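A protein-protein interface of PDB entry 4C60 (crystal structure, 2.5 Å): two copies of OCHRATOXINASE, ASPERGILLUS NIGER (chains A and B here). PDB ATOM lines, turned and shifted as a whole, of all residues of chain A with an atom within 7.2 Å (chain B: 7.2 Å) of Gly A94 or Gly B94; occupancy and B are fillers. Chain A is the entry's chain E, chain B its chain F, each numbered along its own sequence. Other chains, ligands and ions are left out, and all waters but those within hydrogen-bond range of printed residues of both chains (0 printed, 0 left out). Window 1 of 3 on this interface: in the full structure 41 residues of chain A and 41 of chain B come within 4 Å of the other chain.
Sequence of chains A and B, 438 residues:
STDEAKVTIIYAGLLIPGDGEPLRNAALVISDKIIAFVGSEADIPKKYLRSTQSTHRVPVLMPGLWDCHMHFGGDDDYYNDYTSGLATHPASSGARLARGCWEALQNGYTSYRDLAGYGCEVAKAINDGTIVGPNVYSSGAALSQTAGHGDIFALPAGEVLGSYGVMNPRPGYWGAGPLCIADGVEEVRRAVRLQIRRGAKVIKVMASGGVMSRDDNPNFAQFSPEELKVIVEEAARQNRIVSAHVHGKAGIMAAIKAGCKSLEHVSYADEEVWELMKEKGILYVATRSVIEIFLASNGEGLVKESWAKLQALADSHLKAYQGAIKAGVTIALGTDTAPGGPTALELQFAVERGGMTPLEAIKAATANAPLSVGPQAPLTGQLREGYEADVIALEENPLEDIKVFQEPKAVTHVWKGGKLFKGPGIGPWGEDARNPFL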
ATOM      1  N   GLY A  73      20.726 -14.980   4.551  1.00  0.00           N
ATOM      2  CA  GLY A  73      20.611 -13.553   4.293  1.00  0.00           C
ATOM      3  C   GLY A  73      19.214 -13.015   4.482  1.00  0.00           C
ATOM      4  O   GLY A  73      19.024 -12.013   5.157  1.00  0.00           O
ATOM      5  N   GLY A  74      18.245 -13.672   3.853  1.00  0.00           N
ATOM      6  CA  GLY A  74      16.841 -13.255   3.915  1.00  0.00           C
ATOM      7  C   GLY A  74      16.592 -11.842   3.403  1.00  0.00           C
ATOM      8  O   GLY A  74      15.655 -11.166   3.845  1.00  0.00           O
ATOM      9  N   THR A  88      18.621  -4.311   4.567  1.00  0.00           N
ATOM     10  CA  THR A  88      17.487  -5.120   5.016  1.00  0.00           C
ATOM     11  C   THR A  88      17.478  -5.191   6.524  1.00  0.00           C
ATOM     12  O   THR A  88      18.506  -5.466   7.142  1.00  0.00           O
ATOM     13  CB  THR A  88      17.549  -6.553   4.467  1.00  0.00           C
ATOM     14  OG1 THR A  88      17.478  -6.531   3.039  1.00  0.00           O
ATOM     15  CG2 THR A  88      16.394  -7.379   5.004  1.00  0.00           C
ATOM     16  N   HIS A  89      16.329  -4.905   7.118  1.00  0.00           N
ATOM     17  CA  HIS A  89      16.185  -5.039   8.566  1.00  0.00           C
ATOM     18  C   HIS A  89      16.205  -6.539   8.912  1.00  0.00           C
ATOM     19  O   HIS A  89      15.556  -7.313   8.241  1.00  0.00           O
ATOM     20  CB  HIS A  89      14.910  -4.356   9.040  1.00  0.00           C
ATOM     21  CG  HIS A  89      14.870  -4.132  10.511  1.00  0.00           C
ATOM     22  ND1 HIS A  89      14.594  -5.148  11.401  1.00  0.00           N
ATOM     23  CD2 HIS A  89      15.042  -3.016  11.254  1.00  0.00           C
ATOM     24  CE1 HIS A  89      14.588  -4.668  12.628  1.00  0.00           C
ATOM     25  NE2 HIS A  89      14.861  -3.376  12.567  1.00  0.00           N
ATOM     26  N   PRO A  90      17.000  -6.947   9.916  1.00  0.00           N
ATOM     27  CA  PRO A  90      17.101  -8.371  10.254  1.00  0.00           C
ATOM     28  C   PRO A  90      15.775  -9.058  10.625  1.00  0.00           C
ATOM     29  O   PRO A  90      15.629 -10.253  10.360  1.00  0.00           O
ATOM     30  CB  PRO A  90      18.057  -8.402  11.461  1.00  0.00           C
ATOM     31  CG  PRO A  90      18.759  -7.102  11.464  1.00  0.00           C
ATOM     32  CD  PRO A  90      17.832  -6.115  10.809  1.00  0.00           C
ATOM     33  N   ALA A  91      14.821  -8.334  11.210  1.00  0.00           N
ATOM     34  CA  ALA A  91      13.463  -8.869  11.409  1.00  0.00           C
ATOM     35  C   ALA A  91      12.793  -9.316  10.089  1.00  0.00           C
ATOM     36  O   ALA A  91      12.138 -10.361  10.042  1.00  0.00           O
ATOM     37  CB  ALA A  91      12.591  -7.860  12.123  1.00  0.00           C
ATOM     38  N   SER A  92      12.960  -8.538   9.018  1.00  0.00           N
ATOM     39  CA  SER A  92      12.527  -8.977   7.689  1.00  0.00           C
ATOM     40  C   SER A  92      13.293 -10.251   7.287  1.00  0.00           C
ATOM     41  O   SER A  92      12.698 -11.204   6.787  1.00  0.00           O
ATOM     42  CB  SER A  92      12.728  -7.875   6.627  1.00  0.00           C
ATOM     43  OG  SER A  92      12.068  -6.672   6.967  1.00  0.00           O
ATOM     44  N   SER A  93      14.602 -10.258   7.514  1.00  0.00           N
ATOM     45  CA  SER A  93      15.449 -11.397   7.147  1.00  0.00           C
ATOM     46  C   SER A  93      15.005 -12.685   7.822  1.00  0.00           C
ATOM     47  O   SER A  93      14.858 -13.730   7.181  1.00  0.00           O
ATOM     48  CB  SER A  93      16.905 -11.117   7.503  1.00  0.00           C
ATOM     49  OG  SER A  93      17.335  -9.915   6.909  1.00  0.00           O
ATOM     50  N   GLY A  94      14.807 -12.605   9.134  1.00  0.00           N
ATOM     51  CA  GLY A  94      14.454 -13.786   9.944  1.00  0.00           C
ATOM     52  C   GLY A  94      13.149 -14.414   9.546  1.00  0.00           C
ATOM     53  O   GLY A  94      13.032 -15.628   9.484  1.00  0.00           O
ATOM     54  N   ALA A  95      12.179 -13.565   9.222  1.00  0.00           N
ATOM     55  CA  ALA A  95      10.886 -14.036   8.731  1.00  0.00           C
ATOM     56  C   ALA A  95      11.071 -14.828   7.437  1.00  0.00           C
ATOM     57  O   ALA A  95      10.560 -15.933   7.318  1.00  0.00           O
ATOM     58  CB  ALA A  95       9.944 -12.863   8.507  1.00  0.00           C
ATOM     59  N   ARG A  96      11.821 -14.265   6.476  1.00  0.00           N
ATOM     60  CA  ARG A  96      12.101 -14.962   5.208  1.00  0.00           C
ATOM     61  C   ARG A  96      12.855 -16.270   5.424  1.00  0.00           C
ATOM     62  O   ARG A  96      12.504 -17.302   4.857  1.00  0.00           O
ATOM     63  CB  ARG A  96      12.874 -14.069   4.244  1.00  0.00           C
ATOM     64  CG  ARG A  96      12.086 -12.847   3.775  1.00  0.00           C
ATOM     65  CD  ARG A  96      12.576 -12.281   2.432  1.00  0.00           C
ATOM     66  NE  ARG A  96      11.839 -11.060   2.076  1.00  0.00           N
ATOM     67  CZ  ARG A  96      12.144  -9.833   2.513  1.00  0.00           C
ATOM     68  NH1 ARG A  96      13.195  -9.654   3.295  1.00  0.00           N
ATOM     69  NH2 ARG A  96      11.398  -8.784   2.179  1.00  0.00           N
ATOM     70  N   LEU A  97      13.860 -16.247   6.286  1.00  0.00           N
ATOM     71  CA  LEU A  97      14.640 -17.454   6.552  1.00  0.00           C
ATOM     72  C   LEU A  97      13.795 -18.588   7.185  1.00  0.00           C
ATOM     73  O   LEU A  97      14.097 -19.771   7.023  1.00  0.00           O
ATOM     74  CB  LEU A  97      15.839 -17.108   7.433  1.00  0.00           C
ATOM     75  CG  LEU A  97      16.866 -16.224   6.738  1.00  0.00           C
ATOM     76  CD1 LEU A  97      17.843 -15.659   7.768  1.00  0.00           C
ATOM     77  CD2 LEU A  97      17.626 -16.971   5.662  1.00  0.00           C
ATOM     78  N   ALA A  98      12.740 -18.207   7.896  1.00  0.00           N
ATOM     79  CA  ALA A  98      11.843 -19.164   8.487  1.00  0.00           C
ATOM     80  C   ALA A  98      11.155 -19.994   7.414  1.00  0.00           C
ATOM     81  O   ALA A  98      11.058 -21.220   7.552  1.00  0.00           O
ATOM     82  CB  ALA A  98      10.810 -18.458   9.354  1.00  0.00           C
ATOM     83  N   ARG A  99      10.656 -19.346   6.362  1.00  0.00           N
ATOM     84  CA  ARG A  99      10.092 -20.069   5.219  1.00  0.00           C
ATOM     85  C   ARG A  99      11.171 -20.979   4.604  1.00  0.00           C
ATOM     86  O   ARG A  99      10.923 -22.156   4.321  1.00  0.00           O
ATOM     87  CB  ARG A  99       9.551 -19.111   4.160  1.00  0.00           C
ATOM     88  CG  ARG A  99       9.020 -19.778   2.880  1.00  0.00           C
ATOM     89  CD  ARG A  99       7.705 -20.490   3.167  1.00  0.00           C
ATOM     90  NE  ARG A  99       7.059 -21.105   2.010  1.00  0.00           N
ATOM     91  CZ  ARG A  99       6.286 -20.476   1.126  1.00  0.00           C
ATOM     92  NH1 ARG A  99       6.040 -19.185   1.214  1.00  0.00           N
ATOM     93  NH2 ARG A  99       5.757 -21.162   0.137  1.00  0.00           N
ATOM     94  N   GLY A 100      12.358 -20.413   4.377  1.00  0.00           N
ATOM     95  CA  GLY A 100      13.455 -21.137   3.725  1.00  0.00           C
ATOM     96  C   GLY A 100      13.869 -22.377   4.493  1.00  0.00           C
ATOM     97  O   GLY A 100      14.136 -23.421   3.903  1.00  0.00           O
ATOM     98  N   TYR A 118      22.619 -14.875   9.351  1.00  0.00           N
ATOM     99  CA  TYR A 118      21.963 -14.920  10.660  1.00  0.00           C
ATOM    100  C   TYR A 118      21.640 -16.352  11.157  1.00  0.00           C
ATOM    101  O   TYR A 118      20.705 -16.545  11.913  1.00  0.00           O
ATOM    102  CB  TYR A 118      20.692 -14.064  10.589  1.00  0.00           C
ATOM    103  CG  TYR A 118      20.916 -12.618  10.219  1.00  0.00           C
ATOM    104  CD1 TYR A 118      21.650 -11.769  11.055  1.00  0.00           C
ATOM    105  CD2 TYR A 118      20.392 -12.084   9.054  1.00  0.00           C
ATOM    106  CE1 TYR A 118      21.844 -10.430  10.735  1.00  0.00           C
ATOM    107  CE2 TYR A 118      20.597 -10.753   8.711  1.00  0.00           C
ATOM    108  CZ  TYR A 118      21.317  -9.927   9.557  1.00  0.00           C
ATOM    109  OH  TYR A 118      21.527  -8.599   9.216  1.00  0.00           O
ATOM    110  N   VAL A 122      18.836 -17.368  13.919  1.00  0.00           N
ATOM    111  CA  VAL A 122      17.661 -18.117  13.484  1.00  0.00           C
ATOM    112  C   VAL A 122      17.649 -19.499  14.127  1.00  0.00           C
ATOM    113  O   VAL A 122      16.576 -20.057  14.372  1.00  0.00           O
ATOM    114  CB  VAL A 122      17.584 -18.214  11.940  1.00  0.00           C
ATOM    115  CG1 VAL A 122      16.486 -19.170  11.505  1.00  0.00           C
ATOM    116  CG2 VAL A 122      17.355 -16.838  11.328  1.00  0.00           C
ATOM    117  N   ALA A 125      15.454 -19.957  17.167  1.00  0.00           N
ATOM    118  CA  ALA A 125      14.030 -20.173  16.936  1.00  0.00           C
ATOM    119  C   ALA A 125      13.716 -21.610  16.503  1.00  0.00           C
ATOM    120  O   ALA A 125      12.617 -22.110  16.719  1.00  0.00           O
ATOM    121  CB  ALA A 125      13.510 -19.181  15.916  1.00  0.00           C
ATOM    122  N   ILE A 131      10.005 -22.371  15.271  1.00  0.00           N
ATOM    123  CA  ILE A 131       9.941 -22.782  13.872  1.00  0.00           C
ATOM    124  C   ILE A 131      10.629 -24.131  13.669  1.00  0.00           C
ATOM    125  O   ILE A 131      11.072 -24.772  14.622  1.00  0.00           O
ATOM    126  CB  ILE A 131      10.560 -21.733  12.927  1.00  0.00           C
ATOM    127  CG1 ILE A 131      12.040 -21.522  13.240  1.00  0.00           C
ATOM    128  CG2 ILE A 131       9.801 -20.421  13.013  1.00  0.00           C
ATOM    129  CD1 ILE A 131      12.764 -20.689  12.207  1.00  0.00           C
ATOM    130  N   GLY B  73       6.886  -8.766  18.931  1.00  0.00           N
ATOM    131  CA  GLY B  73       8.135  -8.801  19.681  1.00  0.00           C
ATOM    132  C   GLY B  73       9.060  -9.940  19.304  1.00  0.00           C
ATOM    133  O   GLY B  73      10.235  -9.709  19.021  1.00  0.00           O
ATOM    134  N   GLY B  74       8.528 -11.159  19.289  1.00  0.00           N
ATOM    135  CA  GLY B  74       9.294 -12.356  18.927  1.00  0.00           C
ATOM    136  C   GLY B  74      10.483 -12.608  19.838  1.00  0.00           C
ATOM    137  O   GLY B  74      11.493 -13.181  19.414  1.00  0.00           O
ATOM    138  N   THR B  88      17.213  -9.321  22.391  1.00  0.00           N
ATOM    139  CA  THR B  88      16.908 -10.273  21.317  1.00  0.00           C
ATOM    140  C   THR B  88      17.307  -9.681  19.968  1.00  0.00           C
ATOM    141  O   THR B  88      16.964  -8.537  19.660  1.00  0.00           O
ATOM    142  CB  THR B  88      15.403 -10.613  21.267  1.00  0.00           C
ATOM    143  OG1 THR B  88      15.014 -11.234  22.489  1.00  0.00           O
ATOM    144  CG2 THR B  88      15.102 -11.567  20.128  1.00  0.00           C
ATOM    145  N   HIS B  89      18.071 -10.450  19.194  1.00  0.00           N
ATOM    146  CA  HIS B  89      18.444 -10.036  17.857  1.00  0.00           C
ATOM    147  C   HIS B  89      17.169 -10.082  16.999  1.00  0.00           C
ATOM    148  O   HIS B  89      16.411 -11.046  17.078  1.00  0.00           O
ATOM    149  CB  HIS B  89      19.539 -10.931  17.296  1.00  0.00           C
ATOM    150  CG  HIS B  89      20.214 -10.375  16.074  1.00  0.00           C
ATOM    151  ND1 HIS B  89      19.624 -10.389  14.835  1.00  0.00           N
ATOM    152  CD2 HIS B  89      21.426  -9.796  15.902  1.00  0.00           C
ATOM    153  CE1 HIS B  89      20.436  -9.852  13.948  1.00  0.00           C
ATOM    154  NE2 HIS B  89      21.540  -9.481  14.572  1.00  0.00           N
ATOM    155  N   PRO B  90      16.905  -9.024  16.198  1.00  0.00           N
ATOM    156  CA  PRO B  90      15.659  -8.995  15.415  1.00  0.00           C
ATOM    157  C   PRO B  90      15.493 -10.163  14.435  1.00  0.00           C
ATOM    158  O   PRO B  90      14.361 -10.541  14.135  1.00  0.00           O
ATOM    159  CB  PRO B  90      15.739  -7.664  14.667  1.00  0.00           C
ATOM    160  CG  PRO B  90      16.764  -6.841  15.394  1.00  0.00           C
ATOM    161  CD  PRO B  90      17.713  -7.800  16.026  1.00  0.00           C
ATOM    162  N   ALA B  91      16.594 -10.716  13.911  1.00  0.00           N
ATOM    163  CA  ALA B  91      16.534 -11.946  13.091  1.00  0.00           C
ATOM    164  C   ALA B  91      15.901 -13.118  13.833  1.00  0.00           C
ATOM    165  O   ALA B  91      15.094 -13.856  13.264  1.00  0.00           O
ATOM    166  CB  ALA B  91      17.908 -12.328  12.574  1.00  0.00           C
ATOM    167  N   SER B  92      16.237 -13.286  15.105  1.00  0.00           N
ATOM    168  CA  SER B  92      15.523 -14.256  15.949  1.00  0.00           C
ATOM    169  C   SER B  92      14.028 -13.872  16.041  1.00  0.00           C
ATOM    170  O   SER B  92      13.152 -14.725  15.912  1.00  0.00           O
ATOM    171  CB  SER B  92      16.130 -14.336  17.364  1.00  0.00           C
ATOM    172  OG  SER B  92      17.519 -14.646  17.335  1.00  0.00           O
ATOM    173  N   SER B  93      13.747 -12.590  16.260  1.00  0.00           N
ATOM    174  CA  SER B  93      12.371 -12.110  16.398  1.00  0.00           C
ATOM    175  C   SER B  93      11.525 -12.408  15.157  1.00  0.00           C
ATOM    176  O   SER B  93      10.404 -12.923  15.267  1.00  0.00           O
ATOM    177  CB  SER B  93      12.349 -10.598  16.674  1.00  0.00           C
ATOM    178  OG  SER B  93      13.142 -10.280  17.791  1.00  0.00           O
ATOM    179  N   GLY B  94      12.056 -12.058  13.990  1.00  0.00           N
ATOM    180  CA  GLY B  94      11.339 -12.224  12.732  1.00  0.00           C
ATOM    181  C   GLY B  94      10.970 -13.651  12.447  1.00  0.00           C
ATOM    182  O   GLY B  94       9.883 -13.935  11.960  1.00  0.00           O
ATOM    183  N   ALA B  95      11.888 -14.549  12.755  1.00  0.00           N
ATOM    184  CA  ALA B  95      11.658 -15.973  12.564  1.00  0.00           C
ATOM    185  C   ALA B  95      10.484 -16.413  13.416  1.00  0.00           C
ATOM    186  O   ALA B  95       9.566 -17.068  12.923  1.00  0.00           O
ATOM    187  CB  ALA B  95      12.909 -16.772  12.916  1.00  0.00           C
ATOM    188  N   ARG B  96      10.508 -16.042  14.693  1.00  0.00           N
ATOM    189  CA  ARG B  96       9.397 -16.375  15.587  1.00  0.00           C
ATOM    190  C   ARG B  96       8.054 -15.782  15.100  1.00  0.00           C
ATOM    191  O   ARG B  96       7.022 -16.441  15.117  1.00  0.00           O
ATOM    192  CB  ARG B  96       9.704 -15.933  17.031  1.00  0.00           C
ATOM    193  CG  ARG B  96      10.877 -16.680  17.661  1.00  0.00           C
ATOM    194  CD  ARG B  96      10.844 -16.702  19.196  1.00  0.00           C
ATOM    195  NE  ARG B  96      12.043 -17.367  19.720  1.00  0.00           N
ATOM    196  CZ  ARG B  96      13.211 -16.750  19.931  1.00  0.00           C
ATOM    197  NH1 ARG B  96      13.350 -15.455  19.663  1.00  0.00           N
ATOM    198  NH2 ARG B  96      14.258 -17.416  20.408  1.00  0.00           N
ATOM    199  N   LEU B  97       8.083 -14.522  14.683  1.00  0.00           N
ATOM    200  CA  LEU B  97       6.868 -13.844  14.247  1.00  0.00           C
ATOM    201  C   LEU B  97       6.279 -14.489  12.987  1.00  0.00           C
ATOM    202  O   LEU B  97       5.053 -14.447  12.767  1.00  0.00           O
ATOM    203  CB  LEU B  97       7.149 -12.358  14.019  1.00  0.00           C
ATOM    204  CG  LEU B  97       7.469 -11.584  15.304  1.00  0.00           C
ATOM    205  CD1 LEU B  97       8.054 -10.221  14.953  1.00  0.00           C
ATOM    206  CD2 LEU B  97       6.241 -11.405  16.183  1.00  0.00           C
ATOM    207  N   ALA B  98       7.133 -15.140  12.209  1.00  0.00           N
ATOM    208  CA  ALA B  98       6.672 -15.867  11.036  1.00  0.00           C
ATOM    209  C   ALA B  98       5.745 -17.029  11.410  1.00  0.00           C
ATOM    210  O   ALA B  98       4.702 -17.204  10.790  1.00  0.00           O
ATOM    211  CB  ALA B  98       7.858 -16.366  10.223  1.00  0.00           C
ATOM    212  N   ARG B  99       6.116 -17.808  12.421  1.00  0.00           N
ATOM    213  CA  ARG B  99       5.230 -18.857  12.965  1.00  0.00           C
ATOM    214  C   ARG B  99       3.933 -18.261  13.509  1.00  0.00           C
ATOM    215  O   ARG B  99       2.840 -18.706  13.162  1.00  0.00           O
ATOM    216  CB  ARG B  99       5.907 -19.625  14.100  1.00  0.00           C
ATOM    217  CG  ARG B  99       5.022 -20.668  14.773  1.00  0.00           C
ATOM    218  CD  ARG B  99       4.809 -21.853  13.844  1.00  0.00           C
ATOM    219  NE  ARG B  99       4.031 -22.934  14.438  1.00  0.00           N
ATOM    220  CZ  ARG B  99       4.512 -23.901  15.228  1.00  0.00           C
ATOM    221  NH1 ARG B  99       5.796 -23.951  15.573  1.00  0.00           N
ATOM    222  NH2 ARG B  99       3.697 -24.831  15.684  1.00  0.00           N
ATOM    223  N   GLY B 100       4.070 -17.201  14.307  1.00  0.00           N
ATOM    224  CA  GLY B 100       2.922 -16.523  14.882  1.00  0.00           C
ATOM    225  C   GLY B 100       1.929 -15.988  13.852  1.00  0.00           C
ATOM    226  O   GLY B 100       0.716 -16.095  14.034  1.00  0.00           O
ATOM    227  N   TYR B 118       7.992  -5.159  15.400  1.00  0.00           N
ATOM    228  CA  TYR B 118       8.533  -5.252  14.050  1.00  0.00           C
ATOM    229  C   TYR B 118       7.469  -5.560  12.980  1.00  0.00           C
ATOM    230  O   TYR B 118       7.783  -6.107  11.926  1.00  0.00           O
ATOM    231  CB  TYR B 118       9.631  -6.307  14.043  1.00  0.00           C
ATOM    232  CG  TYR B 118      10.779  -6.051  15.001  1.00  0.00           C
ATOM    233  CD1 TYR B 118      11.618  -4.964  14.830  1.00  0.00           C
ATOM    234  CD2 TYR B 118      11.033  -6.918  16.072  1.00  0.00           C
ATOM    235  CE1 TYR B 118      12.681  -4.728  15.706  1.00  0.00           C
ATOM    236  CE2 TYR B 118      12.088  -6.707  16.950  1.00  0.00           C
ATOM    237  CZ  TYR B 118      12.916  -5.612  16.772  1.00  0.00           C
ATOM    238  OH  TYR B 118      13.970  -5.384  17.626  1.00  0.00           O
ATOM    239  N   VAL B 122       8.182  -7.125   9.288  1.00  0.00           N
ATOM    240  CA  VAL B 122       7.659  -8.459   8.986  1.00  0.00           C
ATOM    241  C   VAL B 122       6.613  -8.393   7.871  1.00  0.00           C
ATOM    242  O   VAL B 122       6.454  -9.339   7.110  1.00  0.00           O
ATOM    243  CB  VAL B 122       7.105  -9.146  10.256  1.00  0.00           C
ATOM    244  CG1 VAL B 122       6.385 -10.438   9.912  1.00  0.00           C
ATOM    245  CG2 VAL B 122       8.223  -9.424  11.252  1.00  0.00           C
ATOM    246  N   ALA B 125       7.709  -9.250   4.390  1.00  0.00           N
ATOM    247  CA  ALA B 125       7.823 -10.656   4.040  1.00  0.00           C
ATOM    248  C   ALA B 125       6.456 -11.284   3.738  1.00  0.00           C
ATOM    249  O   ALA B 125       6.377 -12.275   3.017  1.00  0.00           O
ATOM    250  CB  ALA B 125       8.543 -11.408   5.139  1.00  0.00           C
ATOM    251  N   ILE B 131       6.347 -15.257   3.318  1.00  0.00           N
ATOM    252  CA  ILE B 131       5.546 -15.912   4.349  1.00  0.00           C
ATOM    253  C   ILE B 131       4.074 -15.534   4.214  1.00  0.00           C
ATOM    254  O   ILE B 131       3.687 -14.835   3.282  1.00  0.00           O
ATOM    255  CB  ILE B 131       6.033 -15.588   5.772  1.00  0.00           C
ATOM    256  CG1 ILE B 131       5.938 -14.082   6.059  1.00  0.00           C
ATOM    257  CG2 ILE B 131       7.462 -16.081   5.973  1.00  0.00           C
ATOM    258  CD1 ILE B 131       6.184 -13.729   7.510  1.00  0.00           C
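His A89 touches Tyr B118, and with the chains exchanged Tyr A118 touches His B89.
Ala A91 touches Tyr B118, and with the chains exchanged Tyr A118 touches Ala B91.
Gly A94 touches Ala B95, and with the chains exchanged Ala A95 touches Gly B94.
Ala A95 touches Ile B131, and with the chains exchanged Ile A131 touches Ala B95.
Positions printed for both chains: 73, 74, 88, 89, 90, 91, 92, 93, 94, 95, 96, 97, 98, 99, 100, 118, 122, 125 and 131.
Of the 21 pairs that touch across the chains among the printed residues, 20 have their exchanged pair printed and touching as well.
O of Ala B125 sits at hydrogen-bond distance from N of Ile B131, 3.0 Å away.
The backbone carbonyl oxygen (O) of His B89 sits at hydrogen-bond distance from the side-chain hydroxyl (OG) of Ser B93, 3.4 Å away.
The backbone NH (N) of Ala B91 sits at hydrogen-bond distance from a ring nitrogen (ND1) of His B89 (3.2 Å).
A ring nitrogen (ND1) of His A89 lies within hydrogen-bond range of the backbone NH (N) of Ala A91.
The backbone NH of Ile A131 sits at hydrogen-bond distance from the backbone carbonyl oxygen of Ala A125 (3.0 Å).
OG of Ser A93 lies within hydrogen-bond range of O of His A89 (3.4 Å).
Pro A90 touches His B89 (CB to CE1, 3.7 Å).
Gly B94 touches Ala A91 (CA to O, 3.4 Å).
Gly A94 touches Ala B91.
Gly A94 touches Ala B95 (O to CA, 3.4 Å).
Ala A95 touches Ala B95.
Ala A95 touches Ala B125.
Ala A95 touches Ile B131.
Tyr A118 touches His B89 (CE1 to CE1, 3.6 Å).
Ala B91 touches Tyr A118.
Ala B95 touches Ile A131 (O to CG2, 3.4 Å).
Printed residues of chain B within 4 Å of Ala A95: Gly B94 (3.4 Å), Ala B95 (3.7 Å), Ala B98 (3.99 Å), Ala B125 (3.9 Å) and Ile B131 (3.4 Å).
Printed residues of chain A within 4 Å of Ala B98: Ala A95 (3.99 Å) and Ala A98 (3.7 Å).
Of the printed residues of chain B, Ala A98 touches Ala B98 (3.7 Å).
Arg A99 touches none of the printed residues of chain B.
The nearest printed residue of chain B that does not touch Gly A94 is Ala B98 (5.3 Å).
The nearest printed residue of chain A that does not touch Gly B94 is Pro A90 (5.3 Å).
Of the 19 printed residues of chain B, 9 touch a printed residue of chain A.
Printed residues of chain B that touch a printed residue of chain A: His B89, Pro B90, Ala B91, Gly B94, Ala B95, Ala B98, Tyr B118, Ala B125 and Ile B131.
Hydrophobic or aromatic side chains of chain B within 4 Å of the printed part of chain A: His B89, Pro B90, Ala B91, Ala B95, Ala B98, Tyr B118, Ala B125 and Ile B131.
Of the 19 printed residues of chain A, 9 touch a printed residue of chain B.
Along chain A the printed residues that touch a printed residue of chain B span positions 89 to 131.
Among the printed residues, no Asp or Glu carboxylate lies within 4 Å of a Lys or Arg side-chain nitrogen of the other chain.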
